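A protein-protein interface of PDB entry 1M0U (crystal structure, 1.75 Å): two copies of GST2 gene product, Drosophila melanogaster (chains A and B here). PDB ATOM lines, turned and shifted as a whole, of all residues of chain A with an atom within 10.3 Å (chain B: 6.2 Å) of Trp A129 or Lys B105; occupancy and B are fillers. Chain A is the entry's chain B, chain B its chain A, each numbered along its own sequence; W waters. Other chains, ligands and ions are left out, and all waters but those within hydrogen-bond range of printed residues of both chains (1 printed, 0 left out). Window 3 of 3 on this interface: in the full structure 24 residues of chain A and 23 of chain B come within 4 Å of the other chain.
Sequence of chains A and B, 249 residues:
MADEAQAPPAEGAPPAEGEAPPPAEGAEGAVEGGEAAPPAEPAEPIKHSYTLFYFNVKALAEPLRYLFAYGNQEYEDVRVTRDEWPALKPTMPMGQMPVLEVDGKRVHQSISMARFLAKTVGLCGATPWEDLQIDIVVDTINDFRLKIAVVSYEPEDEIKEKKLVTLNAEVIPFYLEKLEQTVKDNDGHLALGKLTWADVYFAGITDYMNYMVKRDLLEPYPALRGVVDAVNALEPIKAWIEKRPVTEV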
ATOM      1  N   CYS A 124       4.770  15.013 -15.632  1.00  0.00           N
ATOM      2  CA  CYS A 124       5.776  14.671 -16.621  1.00  0.00           C
ATOM      3  C   CYS A 124       5.691  13.222 -17.069  1.00  0.00           C
ATOM      4  O   CYS A 124       4.608  12.625 -17.027  1.00  0.00           O
ATOM      5  CB  CYS A 124       7.159  15.018 -16.100  1.00  0.00           C
ATOM      6  SG  CYS A 124       7.331  16.801 -15.972  1.00  0.00           S
ATOM      7  N   GLY A 125       6.821  12.691 -17.531  1.00  0.00           N
ATOM      8  CA  GLY A 125       6.905  11.310 -17.971  1.00  0.00           C
ATOM      9  C   GLY A 125       7.674  10.476 -16.972  1.00  0.00           C
ATOM     10  O   GLY A 125       8.060  10.971 -15.920  1.00  0.00           O
ATOM     11  N   ALA A 126       7.924   9.220 -17.331  1.00  0.00           N
ATOM     12  CA  ALA A 126       8.575   8.265 -16.420  1.00  0.00           C
ATOM     13  C   ALA A 126      10.041   8.045 -16.753  1.00  0.00           C
ATOM     14  O   ALA A 126      10.801   7.481 -15.941  1.00  0.00           O
ATOM     15  CB  ALA A 126       7.818   6.927 -16.446  1.00  0.00           C
ATOM     16  N   THR A 127      10.448   8.472 -17.949  1.00  0.00           N
ATOM     17  CA  THR A 127      11.807   8.270 -18.425  1.00  0.00           C
ATOM     18  C   THR A 127      12.280   9.557 -19.101  1.00  0.00           C
ATOM     19  O   THR A 127      11.448  10.395 -19.436  1.00  0.00           O
ATOM     20  CB  THR A 127      11.866   7.140 -19.472  1.00  0.00           C
ATOM     21  OG1 THR A 127      11.108   7.522 -20.635  1.00  0.00           O
ATOM     22  CG2 THR A 127      11.176   5.850 -18.969  1.00  0.00           C
ATOM     23  N   PRO A 128      13.588   9.707 -19.310  1.00  0.00           N
ATOM     24  CA  PRO A 128      14.112  10.818 -20.125  1.00  0.00           C
ATOM     25  C   PRO A 128      13.498  10.873 -21.534  1.00  0.00           C
ATOM     26  O   PRO A 128      13.176  11.957 -22.013  1.00  0.00           O
ATOM     27  CB  PRO A 128      15.601  10.499 -20.213  1.00  0.00           C
ATOM     28  CG  PRO A 128      15.880   9.792 -18.937  1.00  0.00           C
ATOM     29  CD  PRO A 128      14.683   8.889 -18.749  1.00  0.00           C
ATOM     30  N   TRP A 129      13.324   9.720 -22.180  1.00  0.00           N
ATOM     31  CA  TRP A 129      12.677   9.692 -23.491  1.00  0.00           C
ATOM     32  C   TRP A 129      11.255  10.265 -23.459  1.00  0.00           C
ATOM     33  O   TRP A 129      10.884  11.047 -24.330  1.00  0.00           O
ATOM     34  CB  TRP A 129      12.712   8.260 -24.079  1.00  0.00           C
ATOM     35  CG  TRP A 129      12.013   8.147 -25.385  1.00  0.00           C
ATOM     36  CD1 TRP A 129      10.782   7.597 -25.604  1.00  0.00           C
ATOM     37  CD2 TRP A 129      12.483   8.600 -26.660  1.00  0.00           C
ATOM     38  NE1 TRP A 129      10.457   7.681 -26.935  1.00  0.00           N
ATOM     39  CE2 TRP A 129      11.481   8.296 -27.607  1.00  0.00           C
ATOM     40  CE3 TRP A 129      13.655   9.242 -27.103  1.00  0.00           C
ATOM     41  CZ2 TRP A 129      11.613   8.598 -28.967  1.00  0.00           C
ATOM     42  CZ3 TRP A 129      13.785   9.542 -28.458  1.00  0.00           C
ATOM     43  CH2 TRP A 129      12.769   9.223 -29.370  1.00  0.00           C
ATOM     44  N   GLU A 130      10.453   9.896 -22.458  1.00  0.00           N
ATOM     45  CA  GLU A 130       9.098  10.404 -22.377  1.00  0.00           C
ATOM     46  C   GLU A 130       9.119  11.901 -22.080  1.00  0.00           C
ATOM     47  O   GLU A 130       8.333  12.650 -22.648  1.00  0.00           O
ATOM     48  CB  GLU A 130       8.312   9.700 -21.272  1.00  0.00           C
ATOM     49  CG  GLU A 130       7.878   8.274 -21.668  1.00  0.00           C
ATOM     50  CD  GLU A 130       6.930   7.641 -20.651  1.00  0.00           C
ATOM     51  OE1 GLU A 130       6.620   8.254 -19.616  1.00  0.00           O
ATOM     52  OE2 GLU A 130       6.490   6.492 -20.887  1.00  0.00           O
ATOM     53  N   ASP A 131      10.006  12.306 -21.170  1.00  0.00           N
ATOM     54  CA  ASP A 131      10.103  13.721 -20.805  1.00  0.00           C
ATOM     55  C   ASP A 131      10.491  14.547 -22.038  1.00  0.00           C
ATOM     56  O   ASP A 131       9.970  15.660 -22.220  1.00  0.00           O
ATOM     57  CB  ASP A 131      11.120  13.942 -19.686  1.00  0.00           C
ATOM     58  CG  ASP A 131      10.555  13.633 -18.314  1.00  0.00           C
ATOM     59  OD1 ASP A 131       9.314  13.606 -18.168  1.00  0.00           O
ATOM     60  OD2 ASP A 131      11.279  13.420 -17.321  1.00  0.00           O
ATOM     61  N   LEU A 132      11.343  13.975 -22.882  1.00  0.00           N
ATOM     62  CA  LEU A 132      11.751  14.630 -24.134  1.00  0.00           C
ATOM     63  C   LEU A 132      10.559  14.900 -25.042  1.00  0.00           C
ATOM     64  O   LEU A 132      10.462  15.954 -25.644  1.00  0.00           O
ATOM     65  CB  LEU A 132      12.780  13.771 -24.873  1.00  0.00           C
ATOM     66  CG  LEU A 132      13.180  14.184 -26.297  1.00  0.00           C
ATOM     67  CD1 LEU A 132      13.857  15.590 -26.304  1.00  0.00           C
ATOM     68  CD2 LEU A 132      14.073  13.124 -26.917  1.00  0.00           C
ATOM     69  N   GLN A 133       9.647  13.929 -25.162  1.00  0.00           N
ATOM     70  CA  GLN A 133       8.488  14.144 -26.019  1.00  0.00           C
ATOM     71  C   GLN A 133       7.647  15.325 -25.567  1.00  0.00           C
ATOM     72  O   GLN A 133       7.138  16.089 -26.414  1.00  0.00           O
ATOM     73  CB  GLN A 133       7.593  12.896 -26.101  1.00  0.00           C
ATOM     74  CG  GLN A 133       8.314  11.570 -26.341  1.00  0.00           C
ATOM     75  CD  GLN A 133       9.330  11.582 -27.471  1.00  0.00           C
ATOM     76  OE1 GLN A 133      10.510  11.300 -27.242  1.00  0.00           O
ATOM     77  NE2 GLN A 133       8.882  11.851 -28.684  1.00  0.00           N
ATOM     78  N   ILE A 134       7.473  15.472 -24.247  1.00  0.00           N
ATOM     79  CA  ILE A 134       6.699  16.595 -23.734  1.00  0.00           C
ATOM     80  C   ILE A 134       7.489  17.892 -23.977  1.00  0.00           C
ATOM     81  O   ILE A 134       6.914  18.889 -24.406  1.00  0.00           O
ATOM     82  CB  ILE A 134       6.359  16.476 -22.212  1.00  0.00           C
ATOM     83  CG1 ILE A 134       5.646  15.160 -21.880  1.00  0.00           C
ATOM     84  CG2 ILE A 134       5.434  17.616 -21.797  1.00  0.00           C
ATOM     85  CD1 ILE A 134       5.742  14.799 -20.375  1.00  0.00           C
ATOM     86  N   ASP A 135       8.773  17.870 -23.662  1.00  0.00           N
ATOM     87  CA  ASP A 135       9.639  19.050 -23.829  1.00  0.00           C
ATOM     88  C   ASP A 135       9.549  19.572 -25.262  1.00  0.00           C
ATOM     89  O   ASP A 135       9.433  20.785 -25.482  1.00  0.00           O
ATOM     90  CB  ASP A 135      11.094  18.716 -23.519  1.00  0.00           C
ATOM     91  CG  ASP A 135      11.397  18.681 -22.029  1.00  0.00           C
ATOM     92  OD1 ASP A 135      10.561  19.122 -21.210  1.00  0.00           O
ATOM     93  OD2 ASP A 135      12.482  18.244 -21.591  1.00  0.00           O
ATOM     94  N   ILE A 136       9.604  18.668 -26.235  1.00  0.00           N
ATOM     95  CA  ILE A 136       9.595  19.057 -27.653  1.00  0.00           C
ATOM     96  C   ILE A 136       8.340  19.825 -28.031  1.00  0.00           C
ATOM     97  O   ILE A 136       8.405  20.878 -28.681  1.00  0.00           O
ATOM     98  CB  ILE A 136       9.778  17.816 -28.565  1.00  0.00           C
ATOM     99  CG1 ILE A 136      11.219  17.299 -28.465  1.00  0.00           C
ATOM    100  CG2 ILE A 136       9.429  18.154 -30.051  1.00  0.00           C
ATOM    101  CD1 ILE A 136      11.379  15.936 -29.137  1.00  0.00           C
ATOM    102  N   VAL A 137       7.181  19.318 -27.629  1.00  0.00           N
ATOM    103  CA  VAL A 137       5.933  19.962 -27.999  1.00  0.00           C
ATOM    104  C   VAL A 137       5.755  21.307 -27.284  1.00  0.00           C
ATOM    105  O   VAL A 137       5.248  22.272 -27.861  1.00  0.00           O
ATOM    106  CB  VAL A 137       4.722  18.993 -27.870  1.00  0.00           C
ATOM    107  CG1 VAL A 137       4.394  18.694 -26.412  1.00  0.00           C
ATOM    108  CG2 VAL A 137       3.502  19.543 -28.608  1.00  0.00           C
ATOM    109  N   ALA A 191       1.036  15.128 -25.833  1.00  0.00           N
ATOM    110  CA  ALA A 191       2.195  14.235 -25.710  1.00  0.00           C
ATOM    111  C   ALA A 191       1.846  12.977 -24.933  1.00  0.00           C
ATOM    112  O   ALA A 191       0.976  13.017 -24.059  1.00  0.00           O
ATOM    113  CB  ALA A 191       3.374  14.954 -25.028  1.00  0.00           C
ATOM    114  N   LEU A 192       2.548  11.892 -25.260  1.00  0.00           N
ATOM    115  CA  LEU A 192       2.448  10.604 -24.546  1.00  0.00           C
ATOM    116  C   LEU A 192       1.060   9.981 -24.482  1.00  0.00           C
ATOM    117  O   LEU A 192       0.829   9.106 -23.632  1.00  0.00           O
ATOM    118  CB  LEU A 192       3.003  10.725 -23.112  1.00  0.00           C
ATOM    119  CG  LEU A 192       4.383  11.384 -22.967  1.00  0.00           C
ATOM    120  CD1 LEU A 192       4.814  11.404 -21.503  1.00  0.00           C
ATOM    121  CD2 LEU A 192       5.438  10.693 -23.827  1.00  0.00           C
ATOM    122  N   LYS A 194      -1.560  11.022 -23.187  1.00  0.00           N
ATOM    123  CA  LYS A 194      -2.166  11.197 -21.860  1.00  0.00           C
ATOM    124  C   LYS A 194      -1.969  12.622 -21.356  1.00  0.00           C
ATOM    125  O   LYS A 194      -1.196  13.387 -21.929  1.00  0.00           O
ATOM    126  CB  LYS A 194      -1.573  10.209 -20.853  1.00  0.00           C
ATOM    127  CG  LYS A 194      -0.121  10.433 -20.480  1.00  0.00           C
ATOM    128  CD  LYS A 194       0.443   9.144 -19.972  1.00  0.00           C
ATOM    129  CE  LYS A 194       1.716   9.322 -19.225  1.00  0.00           C
ATOM    130  NZ  LYS A 194       2.290   7.965 -19.003  1.00  0.00           N
ATOM    131  N   THR A 196      -0.402  15.607 -19.718  1.00  0.00           N
ATOM    132  CA  THR A 196       0.944  16.010 -19.293  1.00  0.00           C
ATOM    133  C   THR A 196       0.942  17.527 -19.152  1.00  0.00           C
ATOM    134  O   THR A 196      -0.051  18.211 -19.493  1.00  0.00           O
ATOM    135  CB  THR A 196       2.078  15.665 -20.302  1.00  0.00           C
ATOM    136  OG1 THR A 196       1.936  16.471 -21.491  1.00  0.00           O
ATOM    137  CG2 THR A 196       2.038  14.177 -20.772  1.00  0.00           C
ATOM    138  N   LEU B 100      17.548  14.065 -34.153  1.00  0.00           N
ATOM    139  CA  LEU B 100      18.134  12.857 -33.613  1.00  0.00           C
ATOM    140  C   LEU B 100      17.183  11.721 -33.920  1.00  0.00           C
ATOM    141  O   LEU B 100      15.970  11.881 -33.848  1.00  0.00           O
ATOM    142  CB  LEU B 100      18.308  12.947 -32.096  1.00  0.00           C
ATOM    143  CG  LEU B 100      19.511  13.689 -31.504  1.00  0.00           C
ATOM    144  CD1 LEU B 100      19.428  13.631 -29.975  1.00  0.00           C
ATOM    145  CD2 LEU B 100      20.802  13.062 -31.990  1.00  0.00           C
ATOM    146  N   GLU B 101      17.755  10.586 -34.271  1.00  0.00           N
ATOM    147  CA  GLU B 101      16.985   9.384 -34.507  1.00  0.00           C
ATOM    148  C   GLU B 101      17.455   8.369 -33.498  1.00  0.00           C
ATOM    149  O   GLU B 101      18.639   8.035 -33.446  1.00  0.00           O
ATOM    150  CB  GLU B 101      17.241   8.891 -35.918  1.00  0.00           C
ATOM    151  CG  GLU B 101      16.017   8.353 -36.604  1.00  0.00           C
ATOM    152  CD  GLU B 101      16.332   7.911 -38.015  1.00  0.00           C
ATOM    153  OE1 GLU B 101      15.752   8.456 -38.959  1.00  0.00           O
ATOM    154  OE2 GLU B 101      17.203   7.048 -38.164  1.00  0.00           O
ATOM    155  N   VAL B 102      16.527   7.915 -32.661  1.00  0.00           N
ATOM    156  CA  VAL B 102      16.825   6.944 -31.631  1.00  0.00           C
ATOM    157  C   VAL B 102      15.949   5.727 -31.918  1.00  0.00           C
ATOM    158  O   VAL B 102      14.721   5.805 -31.852  1.00  0.00           O
ATOM    159  CB  VAL B 102      16.549   7.490 -30.225  1.00  0.00           C
ATOM    160  CG1 VAL B 102      17.023   6.514 -29.176  1.00  0.00           C
ATOM    161  CG2 VAL B 102      17.244   8.855 -30.030  1.00  0.00           C
ATOM    162  N   ASP B 103      16.604   4.631 -32.277  1.00  0.00           N
ATOM    163  CA  ASP B 103      15.917   3.418 -32.743  1.00  0.00           C
ATOM    164  C   ASP B 103      14.842   3.726 -33.783  1.00  0.00           C
ATOM    165  O   ASP B 103      13.715   3.219 -33.718  1.00  0.00           O
ATOM    166  CB  ASP B 103      15.366   2.640 -31.547  1.00  0.00           C
ATOM    167  CG  ASP B 103      16.444   2.281 -30.550  1.00  0.00           C
ATOM    168  OD1 ASP B 103      17.575   1.965 -30.968  1.00  0.00           O
ATOM    169  OD2 ASP B 103      16.263   2.294 -29.320  1.00  0.00           O
ATOM    170  N   GLY B 104      15.208   4.581 -34.740  1.00  0.00           N
ATOM    171  CA  GLY B 104      14.307   5.008 -35.797  1.00  0.00           C
ATOM    172  C   GLY B 104      13.404   6.188 -35.465  1.00  0.00           C
ATOM    173  O   GLY B 104      12.991   6.930 -36.366  1.00  0.00           O
ATOM    174  N   LYS B 105      13.094   6.380 -34.185  1.00  0.00           N
ATOM    175  CA  LYS B 105      12.156   7.426 -33.798  1.00  0.00           C
ATOM    176  C   LYS B 105      12.828   8.789 -33.924  1.00  0.00           C
ATOM    177  O   LYS B 105      13.843   9.020 -33.284  1.00  0.00           O
ATOM    178  CB  LYS B 105      11.643   7.197 -32.374  1.00  0.00           C
ATOM    179  CG  LYS B 105      11.160   5.757 -32.117  1.00  0.00           C
ATOM    180  CD  LYS B 105      10.010   5.700 -31.122  1.00  0.00           C
ATOM    181  CE  LYS B 105       9.577   4.253 -30.841  1.00  0.00           C
ATOM    182  NZ  LYS B 105       8.917   4.101 -29.492  1.00  0.00           N
ATOM    183  N   ARG B 106      12.269   9.661 -34.758  1.00  0.00           N
ATOM    184  CA  ARG B 106      12.850  10.995 -34.988  1.00  0.00           C
ATOM    185  C   ARG B 106      12.337  12.066 -34.023  1.00  0.00           C
ATOM    186  O   ARG B 106      11.126  12.212 -33.788  1.00  0.00           O
ATOM    187  CB  ARG B 106      12.640  11.459 -36.425  1.00  0.00           C
ATOM    188  CG  ARG B 106      13.602  10.839 -37.403  1.00  0.00           C
ATOM    189  CD  ARG B 106      13.313  11.163 -38.829  1.00  0.00           C
ATOM    190  NE  ARG B 106      14.289  10.538 -39.719  1.00  0.00           N
ATOM    191  CZ  ARG B 106      14.368  10.777 -41.023  1.00  0.00           C
ATOM    192  NH1 ARG B 106      13.514  11.612 -41.601  1.00  0.00           N
ATOM    193  NH2 ARG B 106      15.292  10.177 -41.757  1.00  0.00           N
ATOM    194  N   VAL B 107      13.279  12.835 -33.487  1.00  0.00           N
ATOM    195  CA  VAL B 107      12.955  13.956 -32.613  1.00  0.00           C
ATOM    196  C   VAL B 107      13.716  15.200 -33.095  1.00  0.00           C
ATOM    197  O   VAL B 107      14.659  15.099 -33.878  1.00  0.00           O
ATOM    198  CB  VAL B 107      13.296  13.658 -31.122  1.00  0.00           C
ATOM    199  CG1 VAL B 107      12.257  12.700 -30.493  1.00  0.00           C
ATOM    200  CG2 VAL B 107      14.692  13.092 -30.965  1.00  0.00           C
ATOM    201  N   PHE B 116      18.022  15.736 -22.988  1.00  0.00           N
ATOM    202  CA  PHE B 116      17.814  14.277 -23.047  1.00  0.00           C
ATOM    203  C   PHE B 116      19.155  13.524 -23.103  1.00  0.00           C
ATOM    204  O   PHE B 116      19.378  12.568 -22.353  1.00  0.00           O
ATOM    205  CB  PHE B 116      16.913  13.905 -24.240  1.00  0.00           C
ATOM    206  CG  PHE B 116      16.978  12.440 -24.598  1.00  0.00           C
ATOM    207  CD1 PHE B 116      16.345  11.489 -23.788  1.00  0.00           C
ATOM    208  CD2 PHE B 116      17.688  12.024 -25.717  1.00  0.00           C
ATOM    209  CE1 PHE B 116      16.426  10.126 -24.104  1.00  0.00           C
ATOM    210  CE2 PHE B 116      17.785  10.661 -26.050  1.00  0.00           C
ATOM    211  CZ  PHE B 116      17.142   9.714 -25.242  1.00  0.00           C
HETATM  212  O   HOH W   1       7.964   6.867 -28.639  1.00  0.00           O
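The backbone carbonyl oxygen of Leu B100 lies within hydrogen-bond range of the backbone NH of Val B107. The side-chain hydroxyl of Thr A127 lies close to the backbone NH of Trp A129, at 3.5 Å. The backbone carbonyl oxygen (O) of Trp A129 sits close to the side-chain amide oxygen (OE1) of Gln A133, 2.9 Å away.
Water W1 lies within hydrogen-bond range of the side-chain amino group (NZ) of Lys B105 (3.0 Å) and the indole nitrogen (NE1) of Trp A129 (3.1 Å).
Pro A128 touches Phe B116 (O to CD1, 3.7 Å). Trp A129 touches Val B102 (CZ3 to CG2, 3.9 Å). Lys B105 touches Trp A129 (CB to CZ2, 3.7 Å). Val B107 touches Trp A129 (CG1 to CH2, 3.7 Å). N of Trp A129 touches CE1 of Phe B116, at 3.7 Å. Leu A132 touches Phe B116. Gln A133 touches Val B107. CB of Val B107 touches CD1 of Ile A136, 3.6 Å away.
Of the 18 printed residues of chain A, 5 touch a printed residue of chain B. Printed residues of chain A that touch a printed residue of chain B: Pro A128, Trp A129, Leu A132, Gln A133 and Ile A136. Hydrophobic or aromatic side chains of chain A that line the printed part of chain B: Pro A128, Trp A129, Leu A132 and Ile A136. Hydrophobic or aromatic side chains of chain B that line the printed part of chain A: Val B102, Val B107 and Phe B116. Along chain B the printed residues that touch a printed residue of chain A span positions 102 to 116. Among the printed residues, 8 pairs touch across the chains.
No position is printed for both chains. Of the 8 pairs that touch across the chains among the printed residues, none has its exchanged pair printed and touching as well.
Cys A124 touches none of the printed residues of chain B. Of the printed residues of chain B, Pro A128 touches Phe B116 (3.7 Å). Of the printed residues of chain B, Leu A132 touches Phe B116. Printed residues of chain B within 4 Å of Gln A133: Val B107 (3.9 Å). Printed residues of chain B within 4 Å of Ile A136: Val B107 (3.6 Å). No residue of chain A comes within 4 Å of Gly B104. Lys B105 touches one residue of chain A. Printed residues of chain A within 4 Å of Phe B116: Pro A128, Trp A129 and Leu A132.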
